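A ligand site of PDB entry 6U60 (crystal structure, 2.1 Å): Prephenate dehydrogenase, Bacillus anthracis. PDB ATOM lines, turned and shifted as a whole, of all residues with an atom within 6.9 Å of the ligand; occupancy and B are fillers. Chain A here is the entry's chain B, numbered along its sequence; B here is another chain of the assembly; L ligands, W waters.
The side-chain carboxylate of Asp 318 is in salt-bridge range of a nitrogen (N1) of the ligand.
O3 of the ligand sits at hydrogen-bond distance from N of Ile 337 of chain B (2.9 Å).
A nitrogen (N1) of the ligand lies within hydrogen-bond range of the backbone carbonyl oxygen of Ile 337 of chain B, at 2.8 Å.
N of Leu 323 is in hydrogen-bond range of O1 of the ligand, 2.9 Å away.
The side-chain amide nitrogen (ND2) of Asn 155 of chain B lies within hydrogen-bond range of an oxygen (O2) of the ligand (3.0 Å).
OG of Ser 336 of chain B is in hydrogen-bond range of N1 of the ligand, 3.1 Å away.
The backbone NH of Ala 322 sits at hydrogen-bond distance from an oxygen (O1) of the ligand, 3.1 Å away.
The side-chain carboxylate (OD2) of Asp 318 sits at hydrogen-bond distance from the side-chain amide nitrogen (ND2) of Asn 155 of chain B (2.8 Å).
The backbone NH (N) of Asp 318 sits at hydrogen-bond distance from the side-chain carboxylate (OE1) of Glu 154 of chain B (3.1 Å).
The backbone NH (N) of Leu 343 is in hydrogen-bond range of the backbone carbonyl oxygen (O) of Val 352 (2.9 Å).
ND2 of Asn 339 of chain B sits at hydrogen-bond distance from O of Ile 342.
O1 of the ligand lies close to O of Lys 319 (3.5 Å).
Val 316 touches the ligand (CG2 to C7, 3.9 Å).
Leu 317 touches the ligand (O to C5, 3.7 Å).
Gly 321 touches the ligand.
CD1 of Ile 342 touches C6 of the ligand, 3.9 Å away.
CG2 of Val 352 touches O2 of the ligand, at 3.6 Å.
Hydrophobic or aromatic side chains that line the ligand: Val 316, Ala 322, Leu 323, Ile 342, Val 352 and Ile 337 of chain B.
Within 4 Å of the ligand: Val 316, Leu 317, Asp 318, Lys 319, Gly 321, Ala 322, Leu 323, Ile 342, Val 352, Asn 155 of chain B, Ser 336 of chain B and Ile 337 of chain B.
The nearest printed residue that does not touch the ligand is Thr 338 of chain B (4.2 Å).
Water W4 lies within hydrogen-bond range of O3 of the ligand (2.6 Å), O of Ile 335 of chain B (2.8 Å) and N of Gly 321 (3.0 Å).
Water W2 lies within hydrogen-bond range of OE1 of Glu 154 of chain B (2.5 Å), O2 of the ligand (2.7 Å) and O of Val 316 (2.8 Å).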
ATOM      1  N   VAL A 316     -20.654  -9.817 -24.139  1.00  0.00           N
ATOM      2  CA  VAL A 316     -21.400  -9.826 -22.843  1.00  0.00           C
ATOM      3  C   VAL A 316     -21.111 -11.143 -22.130  1.00  0.00           C
ATOM      4  O   VAL A 316     -20.922 -12.180 -22.798  1.00  0.00           O
ATOM      5  CB  VAL A 316     -22.919  -9.628 -23.047  1.00  0.00           C
ATOM      6  CG1 VAL A 316     -23.257  -8.207 -23.421  1.00  0.00           C
ATOM      7  CG2 VAL A 316     -23.491 -10.560 -24.074  1.00  0.00           C
ATOM      8  N   LEU A 317     -21.117 -11.093 -20.790  1.00  0.00           N
ATOM      9  CA  LEU A 317     -20.995 -12.256 -19.889  1.00  0.00           C
ATOM     10  C   LEU A 317     -22.374 -12.879 -19.701  1.00  0.00           C
ATOM     11  O   LEU A 317     -23.378 -12.136 -19.612  1.00  0.00           O
ATOM     12  CB  LEU A 317     -20.401 -11.811 -18.554  1.00  0.00           C
ATOM     13  CG  LEU A 317     -18.875 -11.781 -18.483  1.00  0.00           C
ATOM     14  CD1 LEU A 317     -18.438 -11.343 -17.113  1.00  0.00           C
ATOM     15  CD2 LEU A 317     -18.260 -13.144 -18.799  1.00  0.00           C
ATOM     16  N   ASP A 318     -22.410 -14.206 -19.617  1.00  0.00           N
ATOM     17  CA  ASP A 318     -23.670 -14.942 -19.332  1.00  0.00           C
ATOM     18  C   ASP A 318     -24.067 -14.722 -17.854  1.00  0.00           C
ATOM     19  O   ASP A 318     -23.758 -15.579 -17.012  1.00  0.00           O
ATOM     20  CB  ASP A 318     -23.524 -16.411 -19.703  1.00  0.00           C
ATOM     21  CG  ASP A 318     -24.831 -17.182 -19.662  1.00  0.00           C
ATOM     22  OD1 ASP A 318     -25.916 -16.535 -19.434  1.00  0.00           O
ATOM     23  OD2 ASP A 318     -24.774 -18.416 -19.868  1.00  0.00           O
ATOM     24  N   LYS A 319     -24.836 -13.673 -17.601  1.00  0.00           N
ATOM     25  CA  LYS A 319     -25.386 -13.333 -16.268  1.00  0.00           C
ATOM     26  C   LYS A 319     -26.861 -12.964 -16.429  1.00  0.00           C
ATOM     27  O   LYS A 319     -27.226 -12.395 -17.492  1.00  0.00           O
ATOM     28  CB  LYS A 319     -24.685 -12.099 -15.687  1.00  0.00           C
ATOM     29  CG  LYS A 319     -23.174 -12.206 -15.518  1.00  0.00           C
ATOM     30  CD  LYS A 319     -22.708 -13.414 -14.690  1.00  0.00           C
ATOM     31  CE  LYS A 319     -21.670 -13.056 -13.649  1.00  0.00           C
ATOM     32  NZ  LYS A 319     -20.776 -14.205 -13.375  1.00  0.00           N
ATOM     33  N   VAL A 320     -27.658 -13.164 -15.381  1.00  0.00           N
ATOM     34  CA  VAL A 320     -29.025 -12.586 -15.318  1.00  0.00           C
ATOM     35  C   VAL A 320     -28.914 -11.094 -15.623  1.00  0.00           C
ATOM     36  O   VAL A 320     -27.934 -10.440 -15.160  1.00  0.00           O
ATOM     37  CB  VAL A 320     -29.717 -12.863 -13.982  1.00  0.00           C
ATOM     38  CG1 VAL A 320     -30.981 -12.032 -13.810  1.00  0.00           C
ATOM     39  CG2 VAL A 320     -30.014 -14.346 -13.836  1.00  0.00           C
ATOM     40  N   GLY A 321     -29.772 -10.593 -16.515  1.00  0.00           N
ATOM     41  CA  GLY A 321     -29.854  -9.125 -16.773  1.00  0.00           C
ATOM     42  C   GLY A 321     -28.867  -8.601 -17.803  1.00  0.00           C
ATOM     43  O   GLY A 321     -28.892  -7.394 -18.078  1.00  0.00           O
ATOM     44  N   ALA A 322     -27.999  -9.418 -18.409  1.00  0.00           N
ATOM     45  CA  ALA A 322     -27.054  -8.930 -19.438  1.00  0.00           C
ATOM     46  C   ALA A 322     -27.868  -8.337 -20.610  1.00  0.00           C
ATOM     47  O   ALA A 322     -27.582  -7.209 -21.035  1.00  0.00           O
ATOM     48  CB  ALA A 322     -26.134 -10.020 -19.921  1.00  0.00           C
ATOM     49  N   LEU A 323     -28.852  -9.060 -21.146  1.00  0.00           N
ATOM     50  CA  LEU A 323     -29.674  -8.528 -22.268  1.00  0.00           C
ATOM     51  C   LEU A 323     -30.518  -7.338 -21.785  1.00  0.00           C
ATOM     52  O   LEU A 323     -30.683  -6.374 -22.552  1.00  0.00           O
ATOM     53  CB  LEU A 323     -30.548  -9.655 -22.831  1.00  0.00           C
ATOM     54  CG  LEU A 323     -29.797 -10.787 -23.533  1.00  0.00           C
ATOM     55  CD1 LEU A 323     -30.736 -11.922 -23.860  1.00  0.00           C
ATOM     56  CD2 LEU A 323     -29.113 -10.307 -24.777  1.00  0.00           C
ATOM     57  N   ALA A 324     -31.034  -7.387 -20.561  1.00  0.00           N
ATOM     58  CA  ALA A 324     -31.817  -6.280 -19.968  1.00  0.00           C
ATOM     59  C   ALA A 324     -30.995  -4.993 -20.016  1.00  0.00           C
ATOM     60  O   ALA A 324     -31.574  -3.918 -20.379  1.00  0.00           O
ATOM     61  CB  ALA A 324     -32.254  -6.640 -18.576  1.00  0.00           C
ATOM     62  N   HIS A 325     -29.734  -5.044 -19.622  1.00  0.00           N
ATOM     63  CA  HIS A 325     -28.872  -3.831 -19.582  1.00  0.00           C
ATOM     64  C   HIS A 325     -28.607  -3.315 -21.007  1.00  0.00           C
ATOM     65  O   HIS A 325     -28.741  -2.099 -21.216  1.00  0.00           O
ATOM     66  CB  HIS A 325     -27.601  -4.055 -18.738  1.00  0.00           C
ATOM     67  CG  HIS A 325     -26.885  -2.783 -18.392  1.00  0.00           C
ATOM     68  ND1 HIS A 325     -25.502  -2.711 -18.337  1.00  0.00           N
ATOM     69  CD2 HIS A 325     -27.334  -1.531 -18.132  1.00  0.00           C
ATOM     70  CE1 HIS A 325     -25.123  -1.490 -18.033  1.00  0.00           C
ATOM     71  NE2 HIS A 325     -26.235  -0.740 -17.903  1.00  0.00           N
ATOM     72  N   ILE A 342     -28.084 -14.684 -29.625  1.00  0.00           N
ATOM     73  CA  ILE A 342     -26.849 -15.205 -28.979  1.00  0.00           C
ATOM     74  C   ILE A 342     -26.268 -16.242 -29.936  1.00  0.00           C
ATOM     75  O   ILE A 342     -27.033 -17.113 -30.328  1.00  0.00           O
ATOM     76  CB  ILE A 342     -27.216 -15.808 -27.605  1.00  0.00           C
ATOM     77  CG1 ILE A 342     -27.679 -14.705 -26.644  1.00  0.00           C
ATOM     78  CG2 ILE A 342     -26.085 -16.654 -27.024  1.00  0.00           C
ATOM     79  CD1 ILE A 342     -26.542 -13.814 -26.146  1.00  0.00           C
ATOM     80  N   LEU A 343     -24.997 -16.155 -30.313  1.00  0.00           N
ATOM     81  CA  LEU A 343     -24.437 -17.109 -31.314  1.00  0.00           C
ATOM     82  C   LEU A 343     -23.680 -18.211 -30.569  1.00  0.00           C
ATOM     83  O   LEU A 343     -22.840 -17.898 -29.707  1.00  0.00           O
ATOM     84  CB  LEU A 343     -23.541 -16.376 -32.312  1.00  0.00           C
ATOM     85  CG  LEU A 343     -24.206 -15.329 -33.214  1.00  0.00           C
ATOM     86  CD1 LEU A 343     -23.290 -14.942 -34.357  1.00  0.00           C
ATOM     87  CD2 LEU A 343     -25.519 -15.834 -33.777  1.00  0.00           C
ATOM     88  N   ARG A 346     -19.809 -19.526 -33.716  1.00  0.00           N
ATOM     89  CA  ARG A 346     -19.378 -18.137 -34.023  1.00  0.00           C
ATOM     90  C   ARG A 346     -17.876 -18.040 -34.330  1.00  0.00           C
ATOM     91  O   ARG A 346     -17.261 -17.014 -33.984  1.00  0.00           O
ATOM     92  CB  ARG A 346     -19.800 -17.168 -32.912  1.00  0.00           C
ATOM     93  CG  ARG A 346     -19.409 -17.544 -31.501  1.00  0.00           C
ATOM     94  CD  ARG A 346     -19.824 -16.481 -30.465  1.00  0.00           C
ATOM     95  NE  ARG A 346     -19.115 -16.630 -29.209  1.00  0.00           N
ATOM     96  CZ  ARG A 346     -19.494 -17.414 -28.192  1.00  0.00           C
ATOM     97  NH1 ARG A 346     -20.630 -18.105 -28.232  1.00  0.00           N
ATOM     98  NH2 ARG A 346     -18.722 -17.510 -27.117  1.00  0.00           N
ATOM     99  N   VAL A 352     -20.535 -12.438 -28.593  1.00  0.00           N
ATOM    100  CA  VAL A 352     -21.577 -13.482 -28.471  1.00  0.00           C
ATOM    101  C   VAL A 352     -22.963 -12.963 -28.852  1.00  0.00           C
ATOM    102  O   VAL A 352     -23.748 -13.755 -29.360  1.00  0.00           O
ATOM    103  CB  VAL A 352     -21.556 -14.092 -27.070  1.00  0.00           C
ATOM    104  CG1 VAL A 352     -21.998 -13.075 -26.025  1.00  0.00           C
ATOM    105  CG2 VAL A 352     -22.412 -15.353 -27.046  1.00  0.00           C
ATOM    106  N   LEU A 353     -23.256 -11.696 -28.596  1.00  0.00           N
ATOM    107  CA  LEU A 353     -24.584 -11.104 -28.852  1.00  0.00           C
ATOM    108  C   LEU A 353     -24.513 -10.353 -30.169  1.00  0.00           C
ATOM    109  O   LEU A 353     -23.689  -9.394 -30.273  1.00  0.00           O
ATOM    110  CB  LEU A 353     -24.964 -10.188 -27.695  1.00  0.00           C
ATOM    111  CG  LEU A 353     -26.201  -9.326 -27.909  1.00  0.00           C
ATOM    112  CD1 LEU A 353     -27.419 -10.209 -28.108  1.00  0.00           C
ATOM    113  CD2 LEU A 353     -26.386  -8.345 -26.717  1.00  0.00           C
ATOM    114  N   HIS B 151     -13.711 -16.169 -21.176  1.00  0.00           N
ATOM    115  CA  HIS B 151     -15.104 -16.399 -21.670  1.00  0.00           C
ATOM    116  C   HIS B 151     -15.206 -16.355 -23.208  1.00  0.00           C
ATOM    117  O   HIS B 151     -16.329 -16.275 -23.734  1.00  0.00           O
ATOM    118  CB  HIS B 151     -16.057 -15.433 -20.960  1.00  0.00           C
ATOM    119  CG  HIS B 151     -15.941 -14.001 -21.383  1.00  0.00           C
ATOM    120  ND1 HIS B 151     -15.049 -13.107 -20.772  1.00  0.00           N
ATOM    121  CD2 HIS B 151     -16.625 -13.285 -22.312  1.00  0.00           C
ATOM    122  CE1 HIS B 151     -15.191 -11.910 -21.328  1.00  0.00           C
ATOM    123  NE2 HIS B 151     -16.154 -11.988 -22.272  1.00  0.00           N
ATOM    124  N   GLU B 154     -17.557 -19.088 -24.209  1.00  0.00           N
ATOM    125  CA  GLU B 154     -18.745 -19.244 -23.333  1.00  0.00           C
ATOM    126  C   GLU B 154     -19.998 -19.484 -24.173  1.00  0.00           C
ATOM    127  O   GLU B 154     -20.231 -18.706 -25.090  1.00  0.00           O
ATOM    128  CB  GLU B 154     -18.926 -18.050 -22.392  1.00  0.00           C
ATOM    129  CG  GLU B 154     -19.970 -18.276 -21.322  1.00  0.00           C
ATOM    130  CD  GLU B 154     -20.033 -17.153 -20.278  1.00  0.00           C
ATOM    131  OE1 GLU B 154     -20.132 -15.955 -20.665  1.00  0.00           O
ATOM    132  OE2 GLU B 154     -19.997 -17.492 -19.058  1.00  0.00           O
ATOM    133  N   ASN B 155     -20.704 -20.579 -23.888  1.00  0.00           N
ATOM    134  CA  ASN B 155     -21.914 -21.041 -24.622  1.00  0.00           C
ATOM    135  C   ASN B 155     -21.608 -21.275 -26.106  1.00  0.00           C
ATOM    136  O   ASN B 155     -22.584 -21.353 -26.882  1.00  0.00           O
ATOM    137  CB  ASN B 155     -23.062 -20.050 -24.420  1.00  0.00           C
ATOM    138  CG  ASN B 155     -23.462 -19.993 -22.952  1.00  0.00           C
ATOM    139  OD1 ASN B 155     -23.636 -21.038 -22.344  1.00  0.00           O
ATOM    140  ND2 ASN B 155     -23.573 -18.805 -22.377  1.00  0.00           N
ATOM    141  N   ALA B 156     -20.338 -21.449 -26.502  1.00  0.00           N
ATOM    142  CA  ALA B 156     -19.988 -21.956 -27.852  1.00  0.00           C
ATOM    143  C   ALA B 156     -20.004 -23.499 -27.810  1.00  0.00           C
ATOM    144  O   ALA B 156     -19.666 -24.102 -26.746  1.00  0.00           O
ATOM    145  CB  ALA B 156     -18.660 -21.428 -28.326  1.00  0.00           C
ATOM    146  N   THR B 327     -37.116  -8.163 -21.186  1.00  0.00           N
ATOM    147  CA  THR B 327     -35.889  -8.666 -20.530  1.00  0.00           C
ATOM    148  C   THR B 327     -35.818  -8.116 -19.103  1.00  0.00           C
ATOM    149  O   THR B 327     -35.303  -8.802 -18.207  1.00  0.00           O
ATOM    150  CB  THR B 327     -34.649  -8.379 -21.380  1.00  0.00           C
ATOM    151  OG1 THR B 327     -34.572  -6.989 -21.643  1.00  0.00           O
ATOM    152  CG2 THR B 327     -34.663  -9.173 -22.658  1.00  0.00           C
ATOM    153  N   ALA B 331     -35.375 -10.413 -15.906  1.00  0.00           N
ATOM    154  CA  ALA B 331     -34.194 -10.178 -15.027  1.00  0.00           C
ATOM    155  C   ALA B 331     -34.640  -9.944 -13.565  1.00  0.00           C
ATOM    156  O   ALA B 331     -34.030 -10.521 -12.623  1.00  0.00           O
ATOM    157  CB  ALA B 331     -33.338  -9.056 -15.546  1.00  0.00           C
ATOM    158  N   ILE B 335     -34.541 -14.729 -13.833  1.00  0.00           N
ATOM    159  CA  ILE B 335     -34.551 -15.752 -14.912  1.00  0.00           C
ATOM    160  C   ILE B 335     -33.412 -15.447 -15.885  1.00  0.00           C
ATOM    161  O   ILE B 335     -33.398 -14.337 -16.414  1.00  0.00           O
ATOM    162  CB  ILE B 335     -35.928 -15.762 -15.584  1.00  0.00           C
ATOM    163  CG1 ILE B 335     -37.003 -16.115 -14.568  1.00  0.00           C
ATOM    164  CG2 ILE B 335     -35.964 -16.706 -16.766  1.00  0.00           C
ATOM    165  CD1 ILE B 335     -38.401 -15.807 -15.062  1.00  0.00           C
ATOM    166  N   SER B 336     -32.526 -16.411 -16.111  1.00  0.00           N
ATOM    167  CA  SER B 336     -31.450 -16.394 -17.125  1.00  0.00           C
ATOM    168  C   SER B 336     -32.022 -16.799 -18.491  1.00  0.00           C
ATOM    169  O   SER B 336     -32.790 -17.787 -18.567  1.00  0.00           O
ATOM    170  CB  SER B 336     -30.296 -17.276 -16.745  1.00  0.00           C
ATOM    171  OG  SER B 336     -29.122 -16.863 -17.417  1.00  0.00           O
ATOM    172  N   ILE B 337     -31.692 -16.041 -19.528  1.00  0.00           N
ATOM    173  CA  ILE B 337     -32.096 -16.336 -20.936  1.00  0.00           C
ATOM    174  C   ILE B 337     -30.917 -16.990 -21.631  1.00  0.00           C
ATOM    175  O   ILE B 337     -29.808 -16.434 -21.533  1.00  0.00           O
ATOM    176  CB  ILE B 337     -32.539 -15.051 -21.645  1.00  0.00           C
ATOM    177  CG1 ILE B 337     -33.839 -14.499 -21.054  1.00  0.00           C
ATOM    178  CG2 ILE B 337     -32.687 -15.247 -23.131  1.00  0.00           C
ATOM    179  CD1 ILE B 337     -34.032 -13.032 -21.381  1.00  0.00           C
ATOM    180  N   THR B 338     -31.128 -18.101 -22.338  1.00  0.00           N
ATOM    181  CA  THR B 338     -30.018 -18.799 -23.065  1.00  0.00           C
ATOM    182  C   THR B 338     -29.958 -18.259 -24.495  1.00  0.00           C
ATOM    183  O   THR B 338     -28.857 -18.176 -25.070  1.00  0.00           O
ATOM    184  CB  THR B 338     -30.190 -20.316 -23.014  1.00  0.00           C
ATOM    185  OG1 THR B 338     -31.376 -20.569 -23.737  1.00  0.00           O
ATOM    186  CG2 THR B 338     -30.360 -20.873 -21.628  1.00  0.00           C
ATOM    187  N   ASN B 339     -31.101 -17.880 -25.058  1.00  0.00           N
ATOM    188  CA  ASN B 339     -31.135 -17.361 -26.437  1.00  0.00           C
ATOM    189  C   ASN B 339     -32.427 -16.586 -26.647  1.00  0.00           C
ATOM    190  O   ASN B 339     -33.418 -16.781 -25.897  1.00  0.00           O
ATOM    191  CB  ASN B 339     -30.973 -18.438 -27.513  1.00  0.00           C
ATOM    192  CG  ASN B 339     -30.110 -17.913 -28.655  1.00  0.00           C
ATOM    193  OD1 ASN B 339     -30.250 -16.752 -29.066  1.00  0.00           O
ATOM    194  ND2 ASN B 339     -29.136 -18.709 -29.078  1.00  0.00           N
ATOM    195  N   LEU B 340     -32.384 -15.702 -27.622  1.00  0.00           N
ATOM    196  CA  LEU B 340     -33.628 -15.055 -28.113  1.00  0.00           C
ATOM    197  C   LEU B 340     -33.432 -14.616 -29.543  1.00  0.00           C
ATOM    198  O   LEU B 340     -32.260 -14.430 -29.980  1.00  0.00           O
ATOM    199  CB  LEU B 340     -34.082 -13.926 -27.198  1.00  0.00           C
ATOM    200  CG  LEU B 340     -33.298 -12.620 -27.212  1.00  0.00           C
ATOM    201  CD1 LEU B 340     -33.880 -11.710 -26.164  1.00  0.00           C
ATOM    202  CD2 LEU B 340     -31.815 -12.851 -26.970  1.00  0.00           C
HETATM  203  N1  LIG L   1     -28.126 -15.067 -19.741  1.00  0.00           N
HETATM  204  C1  LIG L   1     -28.084 -13.660 -20.252  1.00  0.00           C
HETATM  205  C2  LIG L   1     -29.341 -12.910 -19.820  1.00  0.00           C
HETATM  206  O1  LIG L   1     -29.439 -11.683 -20.049  1.00  0.00           O
HETATM  207  C3  LIG L   1     -27.953 -13.616 -21.777  1.00  0.00           C
HETATM  208  C4  LIG L   1     -26.689 -14.260 -22.269  1.00  0.00           C
HETATM  209  C5  LIG L   1     -25.501 -13.556 -22.313  1.00  0.00           C
HETATM  210  C6  LIG L   1     -26.659 -15.589 -22.670  1.00  0.00           C
HETATM  211  C7  LIG L   1     -24.319 -14.133 -22.735  1.00  0.00           C
HETATM  212  C8  LIG L   1     -25.490 -16.190 -23.098  1.00  0.00           C
HETATM  213  C9  LIG L   1     -24.317 -15.462 -23.137  1.00  0.00           C
HETATM  214  O2  LIG L   1     -23.143 -16.039 -23.546  1.00  0.00           O
HETATM  215  O3  LIG L   1     -30.246 -13.525 -19.227  1.00  0.00           O
HETATM  216  O   HOH W   1     -26.697 -19.257 -23.997  1.00  0.00           O
HETATM  217  O   HOH W   2     -20.721 -14.926 -22.889  1.00  0.00           O
HETATM  218  O   HOH W   3     -31.278  -9.963 -19.393  1.00  0.00           O
HETATM  219  O   HOH W   4     -31.942 -12.348 -17.657  1.00  0.00           O
